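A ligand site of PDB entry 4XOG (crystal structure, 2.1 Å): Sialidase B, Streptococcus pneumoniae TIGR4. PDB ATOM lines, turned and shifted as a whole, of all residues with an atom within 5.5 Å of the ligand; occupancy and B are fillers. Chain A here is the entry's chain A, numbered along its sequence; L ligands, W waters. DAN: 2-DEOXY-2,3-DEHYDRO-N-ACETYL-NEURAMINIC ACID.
The side-chain carboxylate (OD1) of Asp 291 lies within hydrogen-bond range of an oxygen (O4) of the ligand.
The guanidinium group (NH2) of Arg 209 lies within salt-bridge range of an oxygen (O1A) of the ligand, 2.7 Å away.
The guanidinium group of Arg 583 lies within salt-bridge range of an oxygen (O1A) of the ligand (2.7 Å).
O4 of the ligand is in hydrogen-bond range of NH2 of Arg 228 (2.8 Å).
The side-chain hydroxyl (OH) of Tyr 617 sits close to an oxygen (O1B) of the ligand (3.2 Å).
An oxygen (O8) of the ligand sits at hydrogen-bond distance from the side-chain amide nitrogen (ND2) of Asn 316 (2.9 Å).
An oxygen (O7) of the ligand sits at hydrogen-bond distance from the side-chain carboxylate of Asp 234, 2.9 Å away.
O1B of the ligand is in salt-bridge range of NH1 of Arg 521 (3.5 Å).
The guanidinium group of Arg 209 lies within salt-bridge range of the side-chain carboxylate of Asp 234 (3.8 Å).
The guanidinium group (NH2) of Arg 209 sits at hydrogen-bond distance from the side-chain hydroxyl (OG) of Ser 637 (3.1 Å).
NH1 of Arg 583 lies within hydrogen-bond range of OG of Ser 637.
NH2 of Arg 583 is in hydrogen-bond range of O of Gly 554 (2.8 Å).
NH1 of Arg 228 is in salt-bridge range of OD1 of Asp 234, at 3.0 Å.
OD2 of Asp 226 is in salt-bridge range of NH2 of Arg 228 (2.8 Å).
The side-chain carboxylate (OE2) of Glu 505 is in hydrogen-bond range of the side-chain hydroxyl (OH) of Tyr 617, at 3.0 Å.
The guanidinium group (NH2) of Arg 521 is in hydrogen-bond range of the backbone carbonyl oxygen (O) of Gly 554.
Residues that only touch the ligand: Ile 210, Ile 290, Asp 308, Thr 503 and Trp 638.
Hydrophobic or aromatic side chains within 4 Å of the ligand: Ile 210, Ile 290, Tyr 617 and Trp 638.
Water W2 lies within hydrogen-bond range of the backbone carbonyl oxygen of Ser 235 (2.7 Å), an oxygen (O10) of the ligand (2.8 Å) and the backbone NH of Asn 316 (2.9 Å).
Water W1 bridges O of Ser 637 and O1A of the ligand.
Water W3 lies within hydrogen-bond range of OD2 of Asp 234, OD1 of Asn 316 and O7 of the ligand.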
ATOM      1  N   ARG A 209     -26.656   8.161  -4.650  1.00  0.00           N
ATOM      2  CA  ARG A 209     -25.313   7.640  -4.817  1.00  0.00           C
ATOM      3  C   ARG A 209     -24.325   8.599  -4.154  1.00  0.00           C
ATOM      4  O   ARG A 209     -24.659   9.738  -3.873  1.00  0.00           O
ATOM      5  CB  ARG A 209     -24.968   7.486  -6.293  1.00  0.00           C
ATOM      6  CG  ARG A 209     -25.359   6.152  -6.943  1.00  0.00           C
ATOM      7  CD  ARG A 209     -24.340   5.761  -8.054  1.00  0.00           C
ATOM      8  NE  ARG A 209     -23.021   5.484  -7.498  1.00  0.00           N
ATOM      9  CZ  ARG A 209     -21.907   5.321  -8.216  1.00  0.00           C
ATOM     10  NH1 ARG A 209     -21.943   5.393  -9.550  1.00  0.00           N
ATOM     11  NH2 ARG A 209     -20.758   5.068  -7.602  1.00  0.00           N
ATOM     12  N   ILE A 210     -23.113   8.117  -3.949  1.00  0.00           N
ATOM     13  CA  ILE A 210     -22.012   8.948  -3.480  1.00  0.00           C
ATOM     14  C   ILE A 210     -22.234   9.528  -2.071  1.00  0.00           C
ATOM     15  O   ILE A 210     -22.316  10.744  -1.900  1.00  0.00           O
ATOM     16  CB  ILE A 210     -21.674  10.085  -4.470  1.00  0.00           C
ATOM     17  CG1 ILE A 210     -21.901   9.666  -5.941  1.00  0.00           C
ATOM     18  CG2 ILE A 210     -20.233  10.511  -4.283  1.00  0.00           C
ATOM     19  CD1 ILE A 210     -21.091   8.441  -6.410  1.00  0.00           C
ATOM     20  N   ASP A 226     -25.476  12.479  -3.479  1.00  0.00           N
ATOM     21  CA  ASP A 226     -26.089  12.784  -4.760  1.00  0.00           C
ATOM     22  C   ASP A 226     -27.539  12.337  -4.709  1.00  0.00           C
ATOM     23  O   ASP A 226     -27.814  11.134  -4.624  1.00  0.00           O
ATOM     24  CB  ASP A 226     -25.450  11.956  -5.889  1.00  0.00           C
ATOM     25  CG  ASP A 226     -24.109  12.477  -6.362  1.00  0.00           C
ATOM     26  OD1 ASP A 226     -23.353  13.170  -5.615  1.00  0.00           O
ATOM     27  OD2 ASP A 226     -23.785  12.154  -7.517  1.00  0.00           O
ATOM     28  N   ARG A 228     -30.129  11.513  -7.023  1.00  0.00           N
ATOM     29  CA  ARG A 228     -30.159  11.318  -8.473  1.00  0.00           C
ATOM     30  C   ARG A 228     -31.554  10.952  -8.990  1.00  0.00           C
ATOM     31  O   ARG A 228     -32.167   9.960  -8.559  1.00  0.00           O
ATOM     32  CB  ARG A 228     -29.103  10.292  -8.921  1.00  0.00           C
ATOM     33  CG  ARG A 228     -27.685  10.614  -8.411  1.00  0.00           C
ATOM     34  CD  ARG A 228     -26.644   9.657  -9.001  1.00  0.00           C
ATOM     35  NE  ARG A 228     -25.261  10.104  -8.794  1.00  0.00           N
ATOM     36  CZ  ARG A 228     -24.215   9.603  -9.451  1.00  0.00           C
ATOM     37  NH1 ARG A 228     -24.386   8.640 -10.356  1.00  0.00           N
ATOM     38  NH2 ARG A 228     -23.002  10.074  -9.208  1.00  0.00           N
ATOM     39  N   ASP A 234     -24.577   8.745 -13.818  1.00  0.00           N
ATOM     40  CA  ASP A 234     -23.807   9.960 -13.549  1.00  0.00           C
ATOM     41  C   ASP A 234     -24.344  11.060 -14.452  1.00  0.00           C
ATOM     42  O   ASP A 234     -25.087  10.784 -15.394  1.00  0.00           O
ATOM     43  CB  ASP A 234     -22.307   9.800 -13.914  1.00  0.00           C
ATOM     44  CG  ASP A 234     -21.622   8.633 -13.238  1.00  0.00           C
ATOM     45  OD1 ASP A 234     -22.075   8.156 -12.162  1.00  0.00           O
ATOM     46  OD2 ASP A 234     -20.571   8.208 -13.782  1.00  0.00           O
ATOM     47  N   SER A 235     -23.961  12.298 -14.170  1.00  0.00           N
ATOM     48  CA  SER A 235     -24.181  13.398 -15.116  1.00  0.00           C
ATOM     49  C   SER A 235     -23.636  12.977 -16.485  1.00  0.00           C
ATOM     50  O   SER A 235     -22.603  12.318 -16.526  1.00  0.00           O
ATOM     51  CB  SER A 235     -23.437  14.643 -14.638  1.00  0.00           C
ATOM     52  OG  SER A 235     -23.831  14.994 -13.320  1.00  0.00           O
ATOM     53  N   ILE A 290     -22.700  16.855  -8.830  1.00  0.00           N
ATOM     54  CA  ILE A 290     -22.279  15.475  -8.668  1.00  0.00           C
ATOM     55  C   ILE A 290     -20.992  15.389  -7.872  1.00  0.00           C
ATOM     56  O   ILE A 290     -20.109  16.216  -8.057  1.00  0.00           O
ATOM     57  CB  ILE A 290     -22.156  14.761 -10.059  1.00  0.00           C
ATOM     58  CG1 ILE A 290     -21.681  13.323  -9.911  1.00  0.00           C
ATOM     59  CG2 ILE A 290     -21.233  15.547 -11.029  1.00  0.00           C
ATOM     60  CD1 ILE A 290     -21.778  12.555 -11.241  1.00  0.00           C
ATOM     61  N   ASP A 291     -20.928  14.410  -6.972  1.00  0.00           N
ATOM     62  CA  ASP A 291     -19.746  14.117  -6.145  1.00  0.00           C
ATOM     63  C   ASP A 291     -19.468  15.221  -5.133  1.00  0.00           C
ATOM     64  O   ASP A 291     -18.767  16.176  -5.452  1.00  0.00           O
ATOM     65  CB  ASP A 291     -18.505  13.886  -7.013  1.00  0.00           C
ATOM     66  CG  ASP A 291     -18.593  12.639  -7.880  1.00  0.00           C
ATOM     67  OD1 ASP A 291     -19.530  11.828  -7.707  1.00  0.00           O
ATOM     68  OD2 ASP A 291     -17.696  12.457  -8.749  1.00  0.00           O
ATOM     69  N   ASP A 308     -18.945  18.901  -7.781  1.00  0.00           N
ATOM     70  CA  ASP A 308     -18.841  19.263  -9.190  1.00  0.00           C
ATOM     71  C   ASP A 308     -20.165  19.888  -9.646  1.00  0.00           C
ATOM     72  O   ASP A 308     -21.236  19.523  -9.157  1.00  0.00           O
ATOM     73  CB  ASP A 308     -18.553  18.033 -10.081  1.00  0.00           C
ATOM     74  CG  ASP A 308     -17.309  17.260  -9.664  1.00  0.00           C
ATOM     75  OD1 ASP A 308     -16.354  17.855  -9.115  1.00  0.00           O
ATOM     76  OD2 ASP A 308     -17.264  16.026  -9.893  1.00  0.00           O
ATOM     77  N   MET A 310     -22.369  20.682 -13.237  1.00  0.00           N
ATOM     78  CA  MET A 310     -22.464  20.397 -14.671  1.00  0.00           C
ATOM     79  C   MET A 310     -23.562  21.234 -15.312  1.00  0.00           C
ATOM     80  O   MET A 310     -24.703  21.188 -14.876  1.00  0.00           O
ATOM     81  CB  MET A 310     -22.772  18.912 -14.913  1.00  0.00           C
ATOM     82  CG  MET A 310     -21.743  17.948 -14.351  1.00  0.00           C
ATOM     83  SD  MET A 310     -20.168  17.982 -15.208  1.00  0.00           S
ATOM     84  CE  MET A 310     -19.301  16.731 -14.246  1.00  0.00           C
ATOM     85  N   ASN A 316     -19.002  14.186 -17.245  1.00  0.00           N
ATOM     86  CA  ASN A 316     -17.559  14.029 -17.476  1.00  0.00           C
ATOM     87  C   ASN A 316     -17.180  13.473 -18.856  1.00  0.00           C
ATOM     88  O   ASN A 316     -16.062  13.688 -19.315  1.00  0.00           O
ATOM     89  CB  ASN A 316     -16.877  13.254 -16.331  1.00  0.00           C
ATOM     90  CG  ASN A 316     -17.230  11.772 -16.310  1.00  0.00           C
ATOM     91  OD1 ASN A 316     -18.207  11.343 -16.949  1.00  0.00           O
ATOM     92  ND2 ASN A 316     -16.455  10.987 -15.561  1.00  0.00           N
ATOM     93  N   TYR A 453     -11.786  17.159 -10.806  1.00  0.00           N
ATOM     94  CA  TYR A 453     -12.972  16.499 -10.291  1.00  0.00           C
ATOM     95  C   TYR A 453     -12.835  16.303  -8.788  1.00  0.00           C
ATOM     96  O   TYR A 453     -11.835  15.774  -8.316  1.00  0.00           O
ATOM     97  CB  TYR A 453     -13.178  15.158 -11.004  1.00  0.00           C
ATOM     98  CG  TYR A 453     -13.575  15.331 -12.449  1.00  0.00           C
ATOM     99  CD1 TYR A 453     -14.887  15.619 -12.790  1.00  0.00           C
ATOM    100  CD2 TYR A 453     -12.636  15.218 -13.468  1.00  0.00           C
ATOM    101  CE1 TYR A 453     -15.261  15.793 -14.091  1.00  0.00           C
ATOM    102  CE2 TYR A 453     -13.007  15.386 -14.800  1.00  0.00           C
ATOM    103  CZ  TYR A 453     -14.324  15.684 -15.102  1.00  0.00           C
ATOM    104  OH  TYR A 453     -14.755  15.858 -16.395  1.00  0.00           O
ATOM    105  N   TYR A 473      -9.079  15.283  -8.482  1.00  0.00           N
ATOM    106  CA  TYR A 473      -8.251  14.569  -9.469  1.00  0.00           C
ATOM    107  C   TYR A 473      -8.465  15.059 -10.899  1.00  0.00           C
ATOM    108  O   TYR A 473      -9.522  15.590 -11.260  1.00  0.00           O
ATOM    109  CB  TYR A 473      -8.485  13.057  -9.390  1.00  0.00           C
ATOM    110  CG  TYR A 473      -9.866  12.623  -9.822  1.00  0.00           C
ATOM    111  CD1 TYR A 473     -10.917  12.628  -8.916  1.00  0.00           C
ATOM    112  CD2 TYR A 473     -10.117  12.187 -11.117  1.00  0.00           C
ATOM    113  CE1 TYR A 473     -12.192  12.208  -9.293  1.00  0.00           C
ATOM    114  CE2 TYR A 473     -11.394  11.770 -11.507  1.00  0.00           C
ATOM    115  CZ  TYR A 473     -12.426  11.782 -10.588  1.00  0.00           C
ATOM    116  OH  TYR A 473     -13.691  11.387 -10.953  1.00  0.00           O
ATOM    117  N   THR A 503      -9.292   7.571 -12.439  1.00  0.00           N
ATOM    118  CA  THR A 503     -10.290   8.113 -11.537  1.00  0.00           C
ATOM    119  C   THR A 503      -9.679   8.026 -10.136  1.00  0.00           C
ATOM    120  O   THR A 503     -10.015   7.137  -9.351  1.00  0.00           O
ATOM    121  CB  THR A 503     -11.601   7.320 -11.631  1.00  0.00           C
ATOM    122  OG1 THR A 503     -12.019   7.257 -12.998  1.00  0.00           O
ATOM    123  CG2 THR A 503     -12.704   7.993 -10.800  1.00  0.00           C
ATOM    124  N   GLU A 505      -9.837   8.930  -7.148  1.00  0.00           N
ATOM    125  CA  GLU A 505     -10.625   9.400  -6.005  1.00  0.00           C
ATOM    126  C   GLU A 505      -9.803   9.149  -4.753  1.00  0.00           C
ATOM    127  O   GLU A 505      -9.406   8.006  -4.487  1.00  0.00           O
ATOM    128  CB  GLU A 505     -11.984   8.696  -5.961  1.00  0.00           C
ATOM    129  CG  GLU A 505     -12.900   9.060  -7.144  1.00  0.00           C
ATOM    130  CD  GLU A 505     -14.005   8.049  -7.363  1.00  0.00           C
ATOM    131  OE1 GLU A 505     -15.069   8.420  -7.945  1.00  0.00           O
ATOM    132  OE2 GLU A 505     -13.819   6.877  -6.965  1.00  0.00           O
ATOM    133  N   ARG A 521      -7.850   5.616  -5.277  1.00  0.00           N
ATOM    134  CA  ARG A 521      -8.224   4.628  -6.293  1.00  0.00           C
ATOM    135  C   ARG A 521      -7.283   4.719  -7.483  1.00  0.00           C
ATOM    136  O   ARG A 521      -6.834   5.807  -7.833  1.00  0.00           O
ATOM    137  CB  ARG A 521      -9.654   4.964  -6.746  1.00  0.00           C
ATOM    138  CG  ARG A 521     -10.236   4.152  -7.882  1.00  0.00           C
ATOM    139  CD  ARG A 521     -11.596   4.719  -8.237  1.00  0.00           C
ATOM    140  NE  ARG A 521     -12.125   4.188  -9.489  1.00  0.00           N
ATOM    141  CZ  ARG A 521     -13.369   4.411  -9.906  1.00  0.00           C
ATOM    142  NH1 ARG A 521     -14.199   5.144  -9.171  1.00  0.00           N
ATOM    143  NH2 ARG A 521     -13.778   3.889 -11.062  1.00  0.00           N
ATOM    144  N   GLY A 554     -11.597   0.028 -10.383  1.00  0.00           N
ATOM    145  CA  GLY A 554     -11.471   0.573  -9.037  1.00  0.00           C
ATOM    146  C   GLY A 554     -12.767   1.137  -8.478  1.00  0.00           C
ATOM    147  O   GLY A 554     -13.772   1.248  -9.189  1.00  0.00           O
ATOM    148  N   ARG A 583     -17.749  -4.806  -7.518  1.00  0.00           N
ATOM    149  CA  ARG A 583     -17.872  -3.946  -6.327  1.00  0.00           C
ATOM    150  C   ARG A 583     -18.679  -4.716  -5.288  1.00  0.00           C
ATOM    151  O   ARG A 583     -19.898  -4.575  -5.186  1.00  0.00           O
ATOM    152  CB  ARG A 583     -18.501  -2.582  -6.662  1.00  0.00           C
ATOM    153  CG  ARG A 583     -17.685  -1.766  -7.699  1.00  0.00           C
ATOM    154  CD  ARG A 583     -18.143  -0.318  -7.847  1.00  0.00           C
ATOM    155  NE  ARG A 583     -17.102   0.549  -8.424  1.00  0.00           N
ATOM    156  CZ  ARG A 583     -17.321   1.738  -8.989  1.00  0.00           C
ATOM    157  NH1 ARG A 583     -18.553   2.217  -9.082  1.00  0.00           N
ATOM    158  NH2 ARG A 583     -16.292   2.459  -9.461  1.00  0.00           N
ATOM    159  N   TYR A 617     -19.276   2.663  -3.355  1.00  0.00           N
ATOM    160  CA  TYR A 617     -18.807   3.893  -2.713  1.00  0.00           C
ATOM    161  C   TYR A 617     -19.263   3.894  -1.257  1.00  0.00           C
ATOM    162  O   TYR A 617     -20.334   3.356  -0.934  1.00  0.00           O
ATOM    163  CB  TYR A 617     -19.335   5.126  -3.438  1.00  0.00           C
ATOM    164  CG  TYR A 617     -18.559   5.506  -4.691  1.00  0.00           C
ATOM    165  CD1 TYR A 617     -18.195   4.537  -5.625  1.00  0.00           C
ATOM    166  CD2 TYR A 617     -18.234   6.826  -4.960  1.00  0.00           C
ATOM    167  CE1 TYR A 617     -17.504   4.886  -6.793  1.00  0.00           C
ATOM    168  CE2 TYR A 617     -17.562   7.187  -6.116  1.00  0.00           C
ATOM    169  CZ  TYR A 617     -17.198   6.219  -7.028  1.00  0.00           C
ATOM    170  OH  TYR A 617     -16.516   6.585  -8.183  1.00  0.00           O
ATOM    171  N   SER A 637     -22.413  -0.646  -8.011  1.00  0.00           N
ATOM    172  CA  SER A 637     -22.748   0.545  -8.780  1.00  0.00           C
ATOM    173  C   SER A 637     -21.957   0.661 -10.091  1.00  0.00           C
ATOM    174  O   SER A 637     -22.087   1.659 -10.823  1.00  0.00           O
ATOM    175  CB  SER A 637     -22.590   1.808  -7.925  1.00  0.00           C
ATOM    176  OG  SER A 637     -21.245   1.968  -7.526  1.00  0.00           O
ATOM    177  N   TRP A 638     -21.122  -0.332 -10.383  1.00  0.00           N
ATOM    178  CA  TRP A 638     -20.460  -0.419 -11.695  1.00  0.00           C
ATOM    179  C   TRP A 638     -21.260  -1.309 -12.630  1.00  0.00           C
ATOM    180  O   TRP A 638     -21.393  -1.010 -13.817  1.00  0.00           O
ATOM    181  CB  TRP A 638     -19.026  -0.959 -11.563  1.00  0.00           C
ATOM    182  CG  TRP A 638     -18.233  -0.866 -12.851  1.00  0.00           C
ATOM    183  CD1 TRP A 638     -18.090  -1.844 -13.816  1.00  0.00           C
ATOM    184  CD2 TRP A 638     -17.479   0.265 -13.326  1.00  0.00           C
ATOM    185  NE1 TRP A 638     -17.290  -1.381 -14.839  1.00  0.00           N
ATOM    186  CE2 TRP A 638     -16.910  -0.094 -14.560  1.00  0.00           C
ATOM    187  CE3 TRP A 638     -17.231   1.546 -12.802  1.00  0.00           C
ATOM    188  CZ2 TRP A 638     -16.101   0.781 -15.294  1.00  0.00           C
ATOM    189  CZ3 TRP A 638     -16.431   2.417 -13.537  1.00  0.00           C
ATOM    190  CH2 TRP A 638     -15.884   2.036 -14.766  1.00  0.00           C
HETATM  191  C1  DAN L   1     -18.335   5.422 -10.330  1.00  0.00           C
HETATM  192  C2  DAN L   1     -18.367   6.883 -10.407  1.00  0.00           C
HETATM  193  C3  DAN L   1     -19.014   7.721  -9.562  1.00  0.00           C
HETATM  194  C4  DAN L   1     -18.950   9.232  -9.743  1.00  0.00           C
HETATM  195  C5  DAN L   1     -18.494   9.593 -11.162  1.00  0.00           C
HETATM  196  C6  DAN L   1     -17.258   8.761 -11.499  1.00  0.00           C
HETATM  197  C7  DAN L   1     -16.684   9.051 -12.886  1.00  0.00           C
HETATM  198  C8  DAN L   1     -15.408   8.250 -13.228  1.00  0.00           C
HETATM  199  C9  DAN L   1     -15.553   6.757 -13.537  1.00  0.00           C
HETATM  200  C10 DAN L   1     -18.447  11.805 -12.287  1.00  0.00           C
HETATM  201  C11 DAN L   1     -18.135  13.260 -12.076  1.00  0.00           C
HETATM  202  N5  DAN L   1     -18.192  11.021 -11.227  1.00  0.00           N
HETATM  203  O1A DAN L   1     -19.276   4.750  -9.836  1.00  0.00           O
HETATM  204  O1B DAN L   1     -17.314   4.843 -10.804  1.00  0.00           O
HETATM  205  O4  DAN L   1     -20.197   9.894  -9.438  1.00  0.00           O
HETATM  206  O6  DAN L   1     -17.634   7.385 -11.537  1.00  0.00           O
HETATM  207  O7  DAN L   1     -17.698   8.794 -13.874  1.00  0.00           O
HETATM  208  O8  DAN L   1     -14.849   8.823 -14.405  1.00  0.00           O
HETATM  209  O9  DAN L   1     -15.504   5.957 -12.328  1.00  0.00           O
HETATM  210  O10 DAN L   1     -18.886  11.384 -13.364  1.00  0.00           O
HETATM  211  O   HOH W   1     -20.492   3.244 -12.066  1.00  0.00           O
HETATM  212  O   HOH W   2     -20.429  12.934 -15.079  1.00  0.00           O
HETATM  213  O   HOH W   3     -19.864   9.213 -16.012  1.00  0.00           O
